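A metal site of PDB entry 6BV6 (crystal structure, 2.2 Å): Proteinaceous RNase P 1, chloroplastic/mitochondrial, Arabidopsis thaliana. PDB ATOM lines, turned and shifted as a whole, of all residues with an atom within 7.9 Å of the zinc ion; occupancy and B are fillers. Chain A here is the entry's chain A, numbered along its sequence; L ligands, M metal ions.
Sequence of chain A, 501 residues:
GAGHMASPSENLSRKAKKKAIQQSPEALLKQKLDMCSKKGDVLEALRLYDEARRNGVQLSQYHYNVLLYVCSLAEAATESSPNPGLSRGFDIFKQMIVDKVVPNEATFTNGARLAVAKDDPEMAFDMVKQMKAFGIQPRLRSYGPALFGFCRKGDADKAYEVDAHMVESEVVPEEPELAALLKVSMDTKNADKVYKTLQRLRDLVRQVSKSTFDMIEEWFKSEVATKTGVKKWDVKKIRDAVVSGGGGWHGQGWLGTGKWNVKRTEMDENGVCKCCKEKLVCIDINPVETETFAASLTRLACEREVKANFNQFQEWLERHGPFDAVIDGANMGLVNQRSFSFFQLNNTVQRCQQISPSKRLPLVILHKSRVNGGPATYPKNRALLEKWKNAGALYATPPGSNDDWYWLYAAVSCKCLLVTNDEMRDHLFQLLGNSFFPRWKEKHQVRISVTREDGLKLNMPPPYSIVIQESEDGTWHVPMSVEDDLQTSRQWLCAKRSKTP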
ATOM      1  N   ASN A 261      -9.602  16.954 -10.108  1.00  0.00           N
ATOM      2  CA  ASN A 261      -9.329  18.347  -9.697  1.00  0.00           C
ATOM      3  C   ASN A 261     -10.637  18.897  -9.111  1.00  0.00           C
ATOM      4  O   ASN A 261     -11.620  19.075  -9.841  1.00  0.00           O
ATOM      5  CB  ASN A 261      -8.860  19.161 -10.917  1.00  0.00           C
ATOM      6  CG  ASN A 261      -8.245  20.500 -10.520  1.00  0.00           C
ATOM      7  OD1 ASN A 261      -7.376  20.572  -9.638  1.00  0.00           O
ATOM      8  ND2 ASN A 261      -8.670  21.561 -11.196  1.00  0.00           N
ATOM      9  N   LYS A 263     -12.366  21.925  -7.079  1.00  0.00           N
ATOM     10  CA  LYS A 263     -12.260  23.309  -6.600  1.00  0.00           C
ATOM     11  C   LYS A 263     -13.590  23.930  -6.219  1.00  0.00           C
ATOM     12  O   LYS A 263     -14.585  23.744  -6.927  1.00  0.00           O
ATOM     13  CB  LYS A 263     -11.630  24.211  -7.668  1.00  0.00           C
ATOM     14  CG  LYS A 263     -10.191  23.850  -8.008  1.00  0.00           C
ATOM     15  CD  LYS A 263      -9.219  24.237  -6.900  1.00  0.00           C
ATOM     16  CE  LYS A 263      -7.792  23.831  -7.253  1.00  0.00           C
ATOM     17  NZ  LYS A 263      -7.602  22.345  -7.274  1.00  0.00           N
ATOM     18  N   THR A 265     -15.661  27.133  -6.387  1.00  0.00           N
ATOM     19  CA  THR A 265     -15.680  28.210  -7.341  1.00  0.00           C
ATOM     20  C   THR A 265     -17.076  28.872  -7.406  1.00  0.00           C
ATOM     21  O   THR A 265     -17.923  28.686  -6.500  1.00  0.00           O
ATOM     22  CB  THR A 265     -15.167  27.725  -8.716  1.00  0.00           C
ATOM     23  OG1 THR A 265     -15.017  28.834  -9.596  1.00  0.00           O
ATOM     24  CG2 THR A 265     -16.118  26.688  -9.360  1.00  0.00           C
ATOM     25  N   GLU A 266     -17.290  29.677  -8.434  1.00  0.00           N
ATOM     26  CA  GLU A 266     -18.555  30.371  -8.667  1.00  0.00           C
ATOM     27  C   GLU A 266     -18.841  30.326 -10.151  1.00  0.00           C
ATOM     28  O   GLU A 266     -17.913  30.141 -10.951  1.00  0.00           O
ATOM     29  CB  GLU A 266     -18.441  31.839  -8.260  1.00  0.00           C
ATOM     30  CG  GLU A 266     -18.356  32.107  -6.765  1.00  0.00           C
ATOM     31  CD  GLU A 266     -17.958  33.548  -6.425  1.00  0.00           C
ATOM     32  OE1 GLU A 266     -17.604  34.338  -7.337  1.00  0.00           O
ATOM     33  OE2 GLU A 266     -17.988  33.907  -5.233  1.00  0.00           O
ATOM     34  N   MET A 267     -20.114  30.492 -10.497  1.00  0.00           N
ATOM     35  CA  MET A 267     -20.517  30.744 -11.881  1.00  0.00           C
ATOM     36  C   MET A 267     -20.612  32.237 -12.075  1.00  0.00           C
ATOM     37  O   MET A 267     -21.016  32.966 -11.175  1.00  0.00           O
ATOM     38  CB  MET A 267     -21.860  30.093 -12.181  1.00  0.00           C
ATOM     39  CG  MET A 267     -21.913  28.596 -11.914  1.00  0.00           C
ATOM     40  SD  MET A 267     -20.736  27.648 -12.907  1.00  0.00           S
ATOM     41  CE  MET A 267     -19.878  26.846 -11.547  1.00  0.00           C
ATOM     42  N   VAL A 272     -21.018  30.394 -16.779  1.00  0.00           N
ATOM     43  CA  VAL A 272     -19.686  29.910 -17.090  1.00  0.00           C
ATOM     44  C   VAL A 272     -18.903  29.672 -15.795  1.00  0.00           C
ATOM     45  O   VAL A 272     -18.827  30.549 -14.950  1.00  0.00           O
ATOM     46  CB  VAL A 272     -18.923  30.907 -17.997  1.00  0.00           C
ATOM     47  CG1 VAL A 272     -17.471  30.480 -18.168  1.00  0.00           C
ATOM     48  CG2 VAL A 272     -19.631  31.021 -19.342  1.00  0.00           C
ATOM     49  N   CYS A 273     -18.313  28.501 -15.647  1.00  0.00           N
ATOM     50  CA  CYS A 273     -17.542  28.165 -14.454  1.00  0.00           C
ATOM     51  C   CYS A 273     -16.238  28.953 -14.474  1.00  0.00           C
ATOM     52  O   CYS A 273     -15.532  28.942 -15.429  1.00  0.00           O
ATOM     53  CB  CYS A 273     -17.280  26.655 -14.447  1.00  0.00           C
ATOM     54  SG  CYS A 273     -16.235  25.892 -13.197  1.00  0.00           S
ATOM     55  N   LYS A 274     -15.950  29.621 -13.371  1.00  0.00           N
ATOM     56  CA  LYS A 274     -14.752  30.451 -13.239  1.00  0.00           C
ATOM     57  C   LYS A 274     -13.459  29.667 -13.306  1.00  0.00           C
ATOM     58  O   LYS A 274     -12.490  30.115 -13.844  1.00  0.00           O
ATOM     59  CB  LYS A 274     -14.837  31.308 -11.997  1.00  0.00           C
ATOM     60  CG  LYS A 274     -15.658  32.542 -12.223  1.00  0.00           C
ATOM     61  CD  LYS A 274     -15.887  33.296 -10.945  1.00  0.00           C
ATOM     62  CE  LYS A 274     -16.960  34.334 -11.079  1.00  0.00           C
ATOM     63  NZ  LYS A 274     -17.234  34.972  -9.769  1.00  0.00           N
ATOM     64  N   CYS A 275     -13.492  28.493 -12.720  1.00  0.00           N
ATOM     65  CA  CYS A 275     -12.419  27.556 -12.751  1.00  0.00           C
ATOM     66  C   CYS A 275     -12.113  26.817 -14.074  1.00  0.00           C
ATOM     67  O   CYS A 275     -10.988  26.816 -14.502  1.00  0.00           O
ATOM     68  CB  CYS A 275     -12.717  26.511 -11.683  1.00  0.00           C
ATOM     69  SG  CYS A 275     -11.342  25.456 -11.270  1.00  0.00           S
ATOM     70  N   CYS A 276     -13.084  26.229 -14.770  1.00  0.00           N
ATOM     71  CA  CYS A 276     -12.841  25.363 -15.934  1.00  0.00           C
ATOM     72  C   CYS A 276     -13.412  25.947 -17.224  1.00  0.00           C
ATOM     73  O   CYS A 276     -13.208  25.393 -18.291  1.00  0.00           O
ATOM     74  CB  CYS A 276     -13.421  23.951 -15.669  1.00  0.00           C
ATOM     75  SG  CYS A 276     -15.231  23.748 -15.657  1.00  0.00           S
ATOM     76  N   LYS A 277     -14.165  27.056 -17.121  1.00  0.00           N
ATOM     77  CA  LYS A 277     -14.773  27.728 -18.288  1.00  0.00           C
ATOM     78  C   LYS A 277     -15.819  26.892 -19.029  1.00  0.00           C
ATOM     79  O   LYS A 277     -16.083  27.146 -20.189  1.00  0.00           O
ATOM     80  CB  LYS A 277     -13.714  28.220 -19.293  1.00  0.00           C
ATOM     81  CG  LYS A 277     -12.463  28.853 -18.680  1.00  0.00           C
ATOM     82  CD  LYS A 277     -12.804  29.959 -17.699  1.00  0.00           C
ATOM     83  CE  LYS A 277     -11.543  30.526 -17.065  1.00  0.00           C
ATOM     84  NZ  LYS A 277     -11.855  31.701 -16.212  1.00  0.00           N
ATOM     85  N   GLU A 278     -16.417  25.907 -18.362  1.00  0.00           N
ATOM     86  CA  GLU A 278     -17.573  25.229 -18.954  1.00  0.00           C
ATOM     87  C   GLU A 278     -18.824  26.106 -18.737  1.00  0.00           C
ATOM     88  O   GLU A 278     -19.036  26.706 -17.668  1.00  0.00           O
ATOM     89  CB  GLU A 278     -17.758  23.813 -18.390  1.00  0.00           C
ATOM     90  CG  GLU A 278     -19.033  23.122 -18.919  1.00  0.00           C
ATOM     91  CD  GLU A 278     -18.937  21.614 -19.076  1.00  0.00           C
ATOM     92  OE1 GLU A 278     -17.860  21.011 -18.886  1.00  0.00           O
ATOM     93  OE2 GLU A 278     -19.986  21.009 -19.418  1.00  0.00           O
ATOM     94  N   LYS A 279     -19.625  26.204 -19.793  1.00  0.00           N
ATOM     95  CA  LYS A 279     -20.906  26.876 -19.761  1.00  0.00           C
ATOM     96  C   LYS A 279     -21.930  25.852 -19.295  1.00  0.00           C
ATOM     97  O   LYS A 279     -22.133  24.850 -19.976  1.00  0.00           O
ATOM     98  CB  LYS A 279     -21.278  27.398 -21.145  1.00  0.00           C
ATOM     99  CG  LYS A 279     -22.478  28.335 -21.160  1.00  0.00           C
ATOM    100  CD  LYS A 279     -22.833  28.768 -22.572  1.00  0.00           C
ATOM    101  CE  LYS A 279     -24.220  29.401 -22.637  1.00  0.00           C
ATOM    102  NZ  LYS A 279     -24.307  30.636 -21.822  1.00  0.00           N
ATOM    103  N   LEU A 280     -22.581  26.131 -18.181  1.00  0.00           N
ATOM    104  CA  LEU A 280     -23.598  25.280 -17.653  1.00  0.00           C
ATOM    105  C   LEU A 280     -24.833  25.342 -18.514  1.00  0.00           C
ATOM    106  O   LEU A 280     -25.083  26.294 -19.191  1.00  0.00           O
ATOM    107  CB  LEU A 280     -23.958  25.651 -16.242  1.00  0.00           C
ATOM    108  CG  LEU A 280     -22.881  25.373 -15.230  1.00  0.00           C
ATOM    109  CD1 LEU A 280     -23.428  25.637 -13.865  1.00  0.00           C
ATOM    110  CD2 LEU A 280     -22.363  23.976 -15.350  1.00  0.00           C
ATOM    111  N   THR A 475     -17.472  15.731 -16.292  1.00  0.00           N
ATOM    112  CA  THR A 475     -17.240  16.835 -15.344  1.00  0.00           C
ATOM    113  C   THR A 475     -18.515  17.170 -14.551  1.00  0.00           C
ATOM    114  O   THR A 475     -19.608  17.172 -15.122  1.00  0.00           O
ATOM    115  CB  THR A 475     -16.739  18.086 -16.075  1.00  0.00           C
ATOM    116  OG1 THR A 475     -15.576  17.724 -16.820  1.00  0.00           O
ATOM    117  CG2 THR A 475     -16.380  19.196 -15.088  1.00  0.00           C
ATOM    118  N   TRP A 476     -18.348  17.431 -13.256  1.00  0.00           N
ATOM    119  CA  TRP A 476     -19.453  17.670 -12.342  1.00  0.00           C
ATOM    120  C   TRP A 476     -19.398  19.088 -11.788  1.00  0.00           C
ATOM    121  O   TRP A 476     -18.339  19.507 -11.345  1.00  0.00           O
ATOM    122  CB  TRP A 476     -19.448  16.692 -11.161  1.00  0.00           C
ATOM    123  CG  TRP A 476     -19.869  15.293 -11.516  1.00  0.00           C
ATOM    124  CD1 TRP A 476     -19.072  14.290 -12.051  1.00  0.00           C
ATOM    125  CD2 TRP A 476     -21.166  14.713 -11.348  1.00  0.00           C
ATOM    126  NE1 TRP A 476     -19.805  13.143 -12.240  1.00  0.00           N
ATOM    127  CE2 TRP A 476     -21.088  13.366 -11.818  1.00  0.00           C
ATOM    128  CE3 TRP A 476     -22.380  15.179 -10.844  1.00  0.00           C
ATOM    129  CZ2 TRP A 476     -22.192  12.517 -11.810  1.00  0.00           C
ATOM    130  CZ3 TRP A 476     -23.476  14.329 -10.824  1.00  0.00           C
ATOM    131  CH2 TRP A 476     -23.372  13.002 -11.317  1.00  0.00           C
ATOM    132  N   HIS A 477     -20.539  19.786 -11.821  1.00  0.00           N
ATOM    133  CA  HIS A 477     -20.729  21.060 -11.073  1.00  0.00           C
ATOM    134  C   HIS A 477     -21.896  20.943 -10.074  1.00  0.00           C
ATOM    135  O   HIS A 477     -23.021  20.606 -10.452  1.00  0.00           O
ATOM    136  CB  HIS A 477     -20.922  22.208 -12.048  1.00  0.00           C
ATOM    137  CG  HIS A 477     -19.750  22.419 -12.950  1.00  0.00           C
ATOM    138  ND1 HIS A 477     -19.601  21.744 -14.138  1.00  0.00           N
ATOM    139  CD2 HIS A 477     -18.648  23.186 -12.815  1.00  0.00           C
ATOM    140  CE1 HIS A 477     -18.472  22.106 -14.724  1.00  0.00           C
ATOM    141  NE2 HIS A 477     -17.865  22.958 -13.930  1.00  0.00           N
ATOM    142  N   TRP A 492     -20.061  26.878  -5.657  1.00  0.00           N
ATOM    143  CA  TRP A 492     -20.165  25.654  -6.437  1.00  0.00           C
ATOM    144  C   TRP A 492     -18.895  24.815  -6.296  1.00  0.00           C
ATOM    145  O   TRP A 492     -17.804  25.353  -6.152  1.00  0.00           O
ATOM    146  CB  TRP A 492     -20.330  25.946  -7.920  1.00  0.00           C
ATOM    147  CG  TRP A 492     -21.601  26.531  -8.359  1.00  0.00           C
ATOM    148  CD1 TRP A 492     -22.048  27.820  -8.151  1.00  0.00           C
ATOM    149  CD2 TRP A 492     -22.600  25.881  -9.177  1.00  0.00           C
ATOM    150  NE1 TRP A 492     -23.277  28.002  -8.755  1.00  0.00           N
ATOM    151  CE2 TRP A 492     -23.635  26.839  -9.399  1.00  0.00           C
ATOM    152  CE3 TRP A 492     -22.731  24.586  -9.723  1.00  0.00           C
ATOM    153  CZ2 TRP A 492     -24.783  26.549 -10.166  1.00  0.00           C
ATOM    154  CZ3 TRP A 492     -23.864  24.284 -10.475  1.00  0.00           C
ATOM    155  CH2 TRP A 492     -24.880  25.278 -10.705  1.00  0.00           C
ATOM    156  N   LEU A 493     -19.061  23.502  -6.424  1.00  0.00           N
ATOM    157  CA  LEU A 493     -17.948  22.572  -6.587  1.00  0.00           C
ATOM    158  C   LEU A 493     -17.719  22.238  -8.064  1.00  0.00           C
ATOM    159  O   LEU A 493     -18.640  21.814  -8.749  1.00  0.00           O
ATOM    160  CB  LEU A 493     -18.270  21.297  -5.793  1.00  0.00           C
ATOM    161  CG  LEU A 493     -17.127  20.445  -5.211  1.00  0.00           C
ATOM    162  CD1 LEU A 493     -16.198  21.287  -4.323  1.00  0.00           C
ATOM    163  CD2 LEU A 493     -17.722  19.278  -4.439  1.00  0.00           C
ATOM    164  N   CYS A 494     -16.498  22.452  -8.547  1.00  0.00           N
ATOM    165  CA  CYS A 494     -16.050  22.034  -9.883  1.00  0.00           C
ATOM    166  C   CYS A 494     -15.111  20.833  -9.701  1.00  0.00           C
ATOM    167  O   CYS A 494     -14.017  20.969  -9.125  1.00  0.00           O
ATOM    168  CB  CYS A 494     -15.296  23.164 -10.589  1.00  0.00           C
ATOM    169  SG  CYS A 494     -14.693  22.800 -12.264  1.00  0.00           S
ATOM    170  N   ALA A 495     -15.586  19.680 -10.139  1.00  0.00           N
ATOM    171  CA  ALA A 495     -14.853  18.414 -10.112  1.00  0.00           C
ATOM    172  C   ALA A 495     -14.626  17.987 -11.539  1.00  0.00           C
ATOM    173  O   ALA A 495     -15.563  17.603 -12.228  1.00  0.00           O
ATOM    174  CB  ALA A 495     -15.637  17.359  -9.364  1.00  0.00           C
ATOM    175  N   LYS A 496     -13.369  18.062 -11.974  1.00  0.00           N
ATOM    176  CA  LYS A 496     -12.949  17.771 -13.356  1.00  0.00           C
ATOM    177  C   LYS A 496     -11.721  16.862 -13.329  1.00  0.00           C
ATOM    178  O   LYS A 496     -10.796  17.092 -12.524  1.00  0.00           O
ATOM    179  CB  LYS A 496     -12.563  19.087 -14.035  1.00  0.00           C
ATOM    180  CG  LYS A 496     -12.423  19.015 -15.540  1.00  0.00           C
ATOM    181  CD  LYS A 496     -11.959  20.373 -16.064  1.00  0.00           C
ATOM    182  CE  LYS A 496     -11.556  20.277 -17.524  1.00  0.00           C
ATOM    183  NZ  LYS A 496     -12.674  19.766 -18.372  1.00  0.00           N
HETATM  184  O1  LIG L   1      -6.318  25.548 -11.981  1.00  0.00           O
HETATM  185  C1  LIG L   1      -7.418  26.038 -11.353  1.00  0.00           C
HETATM  186  C2  LIG L   1      -8.683  25.540 -11.653  1.00  0.00           C
HETATM  187  C3  LIG L   1      -9.813  26.067 -11.004  1.00  0.00           C
HETATM  188  C4  LIG L   1      -9.613  27.075 -10.046  1.00  0.00           C
HETATM  189  O2  LIG L   1     -10.692  27.586  -9.388  1.00  0.00           O
HETATM  190  C5  LIG L   1      -8.334  27.594  -9.728  1.00  0.00           C
HETATM  191  C6  LIG L   1      -7.218  27.053 -10.403  1.00  0.00           C
HETATM  192  C7  LIG L   1      -5.931  27.529 -10.111  1.00  0.00           C
HETATM  193  C8  LIG L   1      -5.738  28.545  -9.172  1.00  0.00           C
HETATM  194  C9  LIG L   1      -6.825  29.081  -8.490  1.00  0.00           C
HETATM  195  C10 LIG L   1      -8.113  28.605  -8.783  1.00  0.00           C
HETATM  196  O3  LIG L   1      -9.199  29.116  -8.137  1.00  0.00           O
HETATM  197 ZN    ZN M   1     -15.904  23.880 -13.730  1.00  0.00          ZN
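SG of Cys 275 is covalently linked to C3 of the ligand (1.7 Å).
O of Glu 278 lies within hydrogen-bond range of N of Cys 273 (2.8 Å). The backbone carbonyl oxygen (O) of Cys 494 is in hydrogen-bond range of the backbone NH (N) of Lys 263 (2.8 Å). SD of Met 267 lies close to N of Cys 273, 3.8 Å away. The side-chain sulfur (SG) of Cys 276 lies close to the backbone NH (N) of Glu 278 (3.7 Å).
The zinc ion is bound by the side-chain sulfur of Cys 276, the side-chain sulfur of Cys 273, a ring nitrogen (NE2) of His 477 and the side-chain sulfur of Cys 494.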
